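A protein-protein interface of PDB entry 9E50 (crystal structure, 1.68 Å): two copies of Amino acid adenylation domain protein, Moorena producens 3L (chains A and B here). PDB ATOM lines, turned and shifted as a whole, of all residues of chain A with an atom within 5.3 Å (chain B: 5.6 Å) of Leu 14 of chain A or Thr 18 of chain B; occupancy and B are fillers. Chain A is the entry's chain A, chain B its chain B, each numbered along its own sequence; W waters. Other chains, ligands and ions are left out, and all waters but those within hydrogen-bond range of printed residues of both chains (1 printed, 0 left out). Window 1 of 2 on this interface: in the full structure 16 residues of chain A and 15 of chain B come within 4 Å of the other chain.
Leu 14 of chain A touches two residues of chain B. Of the printed residues of chain A, Thr 18 of chain B touches Leu 14 (3.7 Å), Glu 98 (3.5 Å), Met 99 (3.2 Å) and Ile 102 (3.6 Å). Of the printed residues of chain A, Gly 20 of chain B touches Glu 98 (3.5 Å). Of the printed residues of chain A, Leu 14 of chain B touches Ser 15 and Thr 18. Of the printed residues of chain B, Met 99 of chain A touches Thr 18 (3.2 Å). Printed residues of chain B within 4 Å of Glu 98 of chain A: Thr 18 (3.5 Å), Val 19 (3.8 Å) and Gly 20 (3.5 Å). The nearest residue of chain B that does not touch Leu 14 of chain A is Leu 14 of chain B (4.1 Å). The nearest residue of chain A that does not touch Thr 18 of chain B is Glu 95 of chain A (4.3 Å). The nearest printed residue of chain A that does not touch Ser 15 of chain B is Met 99 of chain A (4.8 Å).
Water W1 bridges OE2 of Glu 98 of chain A and O of Phe 17 of chain B.
Among the printed residues, pairs that only touch across the chains: Glu 98 of chain A with Thr 18 of chain B (3.5 Å), Glu 98 of chain A with Gly 20 of chain B (3.5 Å), Glu 95 of chain A with Val 19 of chain B (3.6 Å), Ile 102 of chain A with Thr 18 of chain B (3.6 Å), Leu 14 of chain A with Ser 15 of chain B (3.7 Å), Leu 14 of chain A with Thr 18 of chain B (3.7 Å), Thr 18 of chain A with Leu 14 of chain B (3.7 Å), Glu 98 of chain A with Val 19 of chain B (3.8 Å) and Ser 15 of chain A with Leu 14 of chain B (3.9 Å).
Of the 8 printed residues of chain B, 5 touch a printed residue of chain A. Hydrophobic or aromatic side chains of chain B within 4 Å of the printed part of chain A: Leu 14 and Val 19. Along chain B the printed residues that touch a printed residue of chain A span positions 14 to 20. Printed residues of chain A that touch a printed residue of chain B: Leu 14, Ser 15, Thr 18, Glu 95, Glu 98, Met 99 and Ile 102. Hydrophobic or aromatic side chains of chain A within 4 Å of the printed part of chain B: Leu 14, Met 99 and Ile 102. Among the printed residues, 10 pairs touch across the chains.
N of Met 99 of chain A lies within hydrogen-bond range of O of Thr 18 of chain B (3.2 Å).
Leu 14 of chain A touches Ser 15 of chain B, and with the chains exchanged Ser 15 of chain A touches Leu 14 of chain B. Leu 14 of chain A touches Thr 18 of chain B, and with the chains exchanged Thr 18 of chain A touches Leu 14 of chain B.
The backbone carbonyl oxygen (O) of Ser 15 of chain A sits at hydrogen-bond distance from the side-chain hydroxyl (OG1) of Thr 18 of chain A, 3.0 Å away. The backbone NH (N) of Leu 14 of chain A lies close to the side-chain hydroxyl (OG) of Ser 12 of chain A (3.3 Å). O of Ser 15 of chain B lies within hydrogen-bond range of OG1 of Thr 18 of chain B (2.9 Å). O of Leu 14 of chain B lies close to OG1 of Thr 18 of chain B, 3.4 Å away. N of Ser 15 of chain A sits at hydrogen-bond distance from OG of Ser 12 of chain A (3.1 Å).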
ATOM      1  N   SER A  12      21.110  15.599 -17.115  1.00  0.00           N
ATOM      2  CA  SER A  12      20.064  14.755 -17.682  1.00  0.00           C
ATOM      3  C   SER A  12      20.385  13.277 -17.500  1.00  0.00           C
ATOM      4  O   SER A  12      21.465  12.814 -17.874  1.00  0.00           O
ATOM      5  CB  SER A  12      19.897  15.075 -19.169  1.00  0.00           C
ATOM      6  OG  SER A  12      19.168  14.063 -19.839  1.00  0.00           O
ATOM      7  N   LEU A  13      19.434  12.529 -16.930  1.00  0.00           N
ATOM      8  CA  LEU A  13      19.619  11.087 -16.813  1.00  0.00           C
ATOM      9  C   LEU A  13      19.723  10.437 -18.186  1.00  0.00           C
ATOM     10  O   LEU A  13      20.521   9.517 -18.388  1.00  0.00           O
ATOM     11  CB  LEU A  13      18.471  10.463 -16.014  1.00  0.00           C
ATOM     12  CG  LEU A  13      18.296  10.973 -14.583  1.00  0.00           C
ATOM     13  CD1 LEU A  13      17.144  10.246 -13.889  1.00  0.00           C
ATOM     14  CD2 LEU A  13      19.597  10.808 -13.801  1.00  0.00           C
ATOM     15  N   LEU A  14      18.908  10.893 -19.140  1.00  0.00           N
ATOM     16  CA  LEU A  14      18.993  10.354 -20.493  1.00  0.00           C
ATOM     17  C   LEU A  14      20.385  10.564 -21.079  1.00  0.00           C
ATOM     18  O   LEU A  14      20.960   9.645 -21.672  1.00  0.00           O
ATOM     19  CB  LEU A  14      17.929  10.998 -21.382  1.00  0.00           C
ATOM     20  CG  LEU A  14      17.836  10.461 -22.806  1.00  0.00           C
ATOM     21  CD1 LEU A  14      17.460   8.988 -22.796  1.00  0.00           C
ATOM     22  CD2 LEU A  14      16.829  11.278 -23.601  1.00  0.00           C
ATOM     23  N   SER A  15      20.944  11.764 -20.914  1.00  0.00           N
ATOM     24  CA  SER A  15      22.288  12.028 -21.419  1.00  0.00           C
ATOM     25  C   SER A  15      23.313  11.141 -20.731  1.00  0.00           C
ATOM     26  O   SER A  15      24.171  10.538 -21.386  1.00  0.00           O
ATOM     27  CB  SER A  15      22.640  13.501 -21.227  1.00  0.00           C
ATOM     28  OG  SER A  15      21.911  14.318 -22.123  1.00  0.00           O
ATOM     29  N   LEU A  16      23.234  11.043 -19.401  1.00  0.00           N
ATOM     30  CA  LEU A  16      24.191  10.225 -18.666  1.00  0.00           C
ATOM     31  C   LEU A  16      24.113   8.768 -19.101  1.00  0.00           C
ATOM     32  O   LEU A  16      25.142   8.090 -19.207  1.00  0.00           O
ATOM     33  CB  LEU A  16      23.946  10.356 -17.163  1.00  0.00           C
ATOM     34  CG  LEU A  16      24.210  11.735 -16.563  1.00  0.00           C
ATOM     35  CD1 LEU A  16      23.733  11.773 -15.124  1.00  0.00           C
ATOM     36  CD2 LEU A  16      25.690  12.081 -16.652  1.00  0.00           C
ATOM     37  N   PHE A  17      22.902   8.280 -19.390  1.00  0.00           N
ATOM     38  CA  PHE A  17      22.743   6.904 -19.844  1.00  0.00           C
ATOM     39  C   PHE A  17      23.403   6.680 -21.199  1.00  0.00           C
ATOM     40  O   PHE A  17      24.070   5.660 -21.414  1.00  0.00           O
ATOM     41  CB  PHE A  17      21.262   6.525 -19.922  1.00  0.00           C
ATOM     42  CG  PHE A  17      21.022   5.259 -20.693  1.00  0.00           C
ATOM     43  CD1 PHE A  17      21.237   4.025 -20.097  1.00  0.00           C
ATOM     44  CD2 PHE A  17      20.626   5.300 -22.023  1.00  0.00           C
ATOM     45  CE1 PHE A  17      21.042   2.856 -20.807  1.00  0.00           C
ATOM     46  CE2 PHE A  17      20.439   4.136 -22.736  1.00  0.00           C
ATOM     47  CZ  PHE A  17      20.648   2.910 -22.129  1.00  0.00           C
ATOM     48  N   THR A  18      23.191   7.599 -22.146  1.00  0.00           N
ATOM     49  CA  THR A  18      23.675   7.375 -23.506  1.00  0.00           C
ATOM     50  C   THR A  18      25.191   7.454 -23.621  1.00  0.00           C
ATOM     51  O   THR A  18      25.737   7.014 -24.639  1.00  0.00           O
ATOM     52  CB  THR A  18      23.041   8.367 -24.492  1.00  0.00           C
ATOM     53  OG1 THR A  18      23.432   9.705 -24.163  1.00  0.00           O
ATOM     54  CG2 THR A  18      21.517   8.255 -24.467  1.00  0.00           C
ATOM     55  N   VAL A  19      25.883   7.995 -22.617  1.00  0.00           N
ATOM     56  CA  VAL A  19      27.343   7.991 -22.602  1.00  0.00           C
ATOM     57  C   VAL A  19      27.898   6.939 -21.648  1.00  0.00           C
ATOM     58  O   VAL A  19      29.103   6.929 -21.377  1.00  0.00           O
ATOM     59  CB  VAL A  19      27.910   9.382 -22.269  1.00  0.00           C
ATOM     60  CG1 VAL A  19      27.464  10.398 -23.304  1.00  0.00           C
ATOM     61  CG2 VAL A  19      27.500   9.818 -20.870  1.00  0.00           C
ATOM     62  N   TRP A  59      12.506  11.721 -18.081  1.00  0.00           N
ATOM     63  CA  TRP A  59      13.047  10.735 -17.149  1.00  0.00           C
ATOM     64  C   TRP A  59      13.561  11.472 -15.918  1.00  0.00           C
ATOM     65  O   TRP A  59      14.603  12.138 -15.973  1.00  0.00           O
ATOM     66  CB  TRP A  59      14.150   9.931 -17.828  1.00  0.00           C
ATOM     67  CG  TRP A  59      14.768   8.863 -16.978  1.00  0.00           C
ATOM     68  CD1 TRP A  59      14.340   8.419 -15.759  1.00  0.00           C
ATOM     69  CD2 TRP A  59      15.932   8.103 -17.297  1.00  0.00           C
ATOM     70  NE1 TRP A  59      15.172   7.428 -15.297  1.00  0.00           N
ATOM     71  CE2 TRP A  59      16.156   7.211 -16.226  1.00  0.00           C
ATOM     72  CE3 TRP A  59      16.807   8.085 -18.389  1.00  0.00           C
ATOM     73  CZ2 TRP A  59      17.224   6.312 -16.213  1.00  0.00           C
ATOM     74  CZ3 TRP A  59      17.867   7.193 -18.375  1.00  0.00           C
ATOM     75  CH2 TRP A  59      18.067   6.320 -17.292  1.00  0.00           C
ATOM     76  N   GLU A  95       5.315   7.029 -27.199  1.00  0.00           N
ATOM     77  CA  GLU A  95       6.576   7.761 -27.219  1.00  0.00           C
ATOM     78  C   GLU A  95       7.403   7.481 -25.965  1.00  0.00           C
ATOM     79  O   GLU A  95       8.612   7.231 -26.052  1.00  0.00           O
ATOM     80  CB  GLU A  95       6.298   9.257 -27.382  1.00  0.00           C
ATOM     81  CG  GLU A  95       5.756   9.595 -28.773  1.00  0.00           C
ATOM     82  CD  GLU A  95       5.142  10.978 -28.869  1.00  0.00           C
ATOM     83  OE1 GLU A  95       5.354  11.790 -27.945  1.00  0.00           O
ATOM     84  OE2 GLU A  95       4.442  11.249 -29.872  1.00  0.00           O
ATOM     85  N   GLU A  98       8.959   3.991 -26.110  1.00  0.00           N
ATOM     86  CA  GLU A  98      10.158   3.883 -26.933  1.00  0.00           C
ATOM     87  C   GLU A  98      11.390   4.331 -26.157  1.00  0.00           C
ATOM     88  O   GLU A  98      12.426   3.653 -26.181  1.00  0.00           O
ATOM     89  CB  GLU A  98      10.007   4.685 -28.228  1.00  0.00           C
ATOM     90  CG  GLU A  98      11.099   4.340 -29.243  1.00  0.00           C
ATOM     91  CD  GLU A  98      10.803   4.847 -30.640  1.00  0.00           C
ATOM     92  OE1 GLU A  98       9.607   5.008 -30.970  1.00  0.00           O
ATOM     93  OE2 GLU A  98      11.768   5.084 -31.406  1.00  0.00           O
ATOM     94  N   MET A  99      11.284   5.452 -25.430  1.00  0.00           N
ATOM     95  CA  MET A  99      12.388   5.880 -24.573  1.00  0.00           C
ATOM     96  C   MET A  99      12.694   4.833 -23.508  1.00  0.00           C
ATOM     97  O   MET A  99      13.862   4.498 -23.271  1.00  0.00           O
ATOM     98  CB  MET A  99      12.074   7.228 -23.920  1.00  0.00           C
ATOM     99  CG  MET A  99      13.069   7.633 -22.830  1.00  0.00           C
ATOM    100  SD  MET A  99      12.611   9.147 -21.955  1.00  0.00           S
ATOM    101  CE  MET A  99      12.933  10.369 -23.214  1.00  0.00           C
ATOM    102  N   ILE A 102      14.726   1.997 -24.867  1.00  0.00           N
ATOM    103  CA  ILE A 102      16.109   2.366 -25.151  1.00  0.00           C
ATOM    104  C   ILE A 102      16.950   2.326 -23.879  1.00  0.00           C
ATOM    105  O   ILE A 102      18.118   1.912 -23.906  1.00  0.00           O
ATOM    106  CB  ILE A 102      16.150   3.748 -25.828  1.00  0.00           C
ATOM    107  CG1 ILE A 102      15.611   3.636 -27.257  1.00  0.00           C
ATOM    108  CG2 ILE A 102      17.557   4.343 -25.791  1.00  0.00           C
ATOM    109  CD1 ILE A 102      15.437   4.964 -27.945  1.00  0.00           C
ATOM    110  N   ILE A 103      16.379   2.732 -22.744  1.00  0.00           N
ATOM    111  CA  ILE A 103      17.168   2.797 -21.516  1.00  0.00           C
ATOM    112  C   ILE A 103      17.115   1.476 -20.754  1.00  0.00           C
ATOM    113  O   ILE A 103      17.644   1.378 -19.642  1.00  0.00           O
ATOM    114  CB  ILE A 103      16.739   3.972 -20.611  1.00  0.00           C
ATOM    115  CG1 ILE A 103      15.321   3.778 -20.077  1.00  0.00           C
ATOM    116  CG2 ILE A 103      16.872   5.301 -21.347  1.00  0.00           C
ATOM    117  CD1 ILE A 103      14.898   4.867 -19.108  1.00  0.00           C
ATOM    118  N   LEU B  13      17.810  17.199 -29.320  1.00  0.00           N
ATOM    119  CA  LEU B  13      17.753  16.235 -30.415  1.00  0.00           C
ATOM    120  C   LEU B  13      17.800  14.810 -29.881  1.00  0.00           C
ATOM    121  O   LEU B  13      17.126  13.915 -30.406  1.00  0.00           O
ATOM    122  CB  LEU B  13      18.896  16.483 -31.405  1.00  0.00           C
ATOM    123  CG  LEU B  13      18.982  17.871 -32.051  1.00  0.00           C
ATOM    124  CD1 LEU B  13      20.089  17.936 -33.109  1.00  0.00           C
ATOM    125  CD2 LEU B  13      17.641  18.276 -32.660  1.00  0.00           C
ATOM    126  N   LEU B  14      18.585  14.586 -28.824  1.00  0.00           N
ATOM    127  CA  LEU B  14      18.637  13.273 -28.188  1.00  0.00           C
ATOM    128  C   LEU B  14      17.261  12.853 -27.678  1.00  0.00           C
ATOM    129  O   LEU B  14      16.835  11.710 -27.880  1.00  0.00           O
ATOM    130  CB  LEU B  14      19.655  13.294 -27.048  1.00  0.00           C
ATOM    131  CG  LEU B  14      19.944  11.956 -26.364  1.00  0.00           C
ATOM    132  CD1 LEU B  14      20.604  10.992 -27.338  1.00  0.00           C
ATOM    133  CD2 LEU B  14      20.811  12.159 -25.130  1.00  0.00           C
ATOM    134  N   SER B  15      16.551  13.765 -27.007  1.00  0.00           N
ATOM    135  CA  SER B  15      15.222  13.424 -26.506  1.00  0.00           C
ATOM    136  C   SER B  15      14.259  13.151 -27.651  1.00  0.00           C
ATOM    137  O   SER B  15      13.500  12.175 -27.612  1.00  0.00           O
ATOM    138  CB  SER B  15      14.687  14.540 -25.612  1.00  0.00           C
ATOM    139  OG  SER B  15      15.364  14.555 -24.366  1.00  0.00           O
ATOM    140  N   LEU B  16      14.283  13.996 -28.685  1.00  0.00           N
ATOM    141  CA  LEU B  16      13.407  13.784 -29.835  1.00  0.00           C
ATOM    142  C   LEU B  16      13.680  12.440 -30.494  1.00  0.00           C
ATOM    143  O   LEU B  16      12.751  11.754 -30.938  1.00  0.00           O
ATOM    144  CB  LEU B  16      13.579  14.920 -30.840  1.00  0.00           C
ATOM    145  CG  LEU B  16      13.034  16.288 -30.435  1.00  0.00           C
ATOM    146  CD1 LEU B  16      13.463  17.334 -31.446  1.00  0.00           C
ATOM    147  CD2 LEU B  16      11.518  16.234 -30.325  1.00  0.00           C
ATOM    148  N   PHE B  17      14.952  12.041 -30.566  1.00  0.00           N
ATOM    149  CA  PHE B  17      15.273  10.751 -31.161  1.00  0.00           C
ATOM    150  C   PHE B  17      14.729   9.597 -30.329  1.00  0.00           C
ATOM    151  O   PHE B  17      14.214   8.617 -30.879  1.00  0.00           O
ATOM    152  CB  PHE B  17      16.786  10.587 -31.333  1.00  0.00           C
ATOM    153  CG  PHE B  17      17.189   9.167 -31.596  1.00  0.00           C
ATOM    154  CD1 PHE B  17      17.067   8.628 -32.863  1.00  0.00           C
ATOM    155  CD2 PHE B  17      17.643   8.357 -30.569  1.00  0.00           C
ATOM    156  CE1 PHE B  17      17.404   7.316 -33.106  1.00  0.00           C
ATOM    157  CE2 PHE B  17      17.981   7.044 -30.804  1.00  0.00           C
ATOM    158  CZ  PHE B  17      17.864   6.522 -32.076  1.00  0.00           C
ATOM    159  N   THR B  18      14.855   9.680 -29.004  1.00  0.00           N
ATOM    160  CA  THR B  18      14.507   8.528 -28.182  1.00  0.00           C
ATOM    161  C   THR B  18      13.004   8.274 -28.143  1.00  0.00           C
ATOM    162  O   THR B  18      12.593   7.177 -27.759  1.00  0.00           O
ATOM    163  CB  THR B  18      15.049   8.691 -26.758  1.00  0.00           C
ATOM    164  OG1 THR B  18      14.548   9.901 -26.182  1.00  0.00           O
ATOM    165  CG2 THR B  18      16.578   8.729 -26.764  1.00  0.00           C
ATOM    166  N   VAL B  19      12.179   9.244 -28.544  1.00  0.00           N
ATOM    167  CA  VAL B  19      10.735   9.040 -28.618  1.00  0.00           C
ATOM    168  C   VAL B  19      10.267   8.788 -30.046  1.00  0.00           C
ATOM    169  O   VAL B  19       9.058   8.724 -30.294  1.00  0.00           O
ATOM    170  CB  VAL B  19       9.967  10.214 -27.986  1.00  0.00           C
ATOM    171  CG1 VAL B  19      10.321  10.327 -26.521  1.00  0.00           C
ATOM    172  CG2 VAL B  19      10.258  11.527 -28.714  1.00  0.00           C
ATOM    173  N   GLY B  20      11.193   8.636 -30.991  1.00  0.00           N
ATOM    174  CA  GLY B  20      10.826   8.356 -32.362  1.00  0.00           C
ATOM    175  C   GLY B  20      10.388   9.552 -33.177  1.00  0.00           C
ATOM    176  O   GLY B  20       9.871   9.367 -34.284  1.00  0.00           O
HETATM  177  O   HOH W   1      14.304   5.836 -31.470  1.00  0.00           O
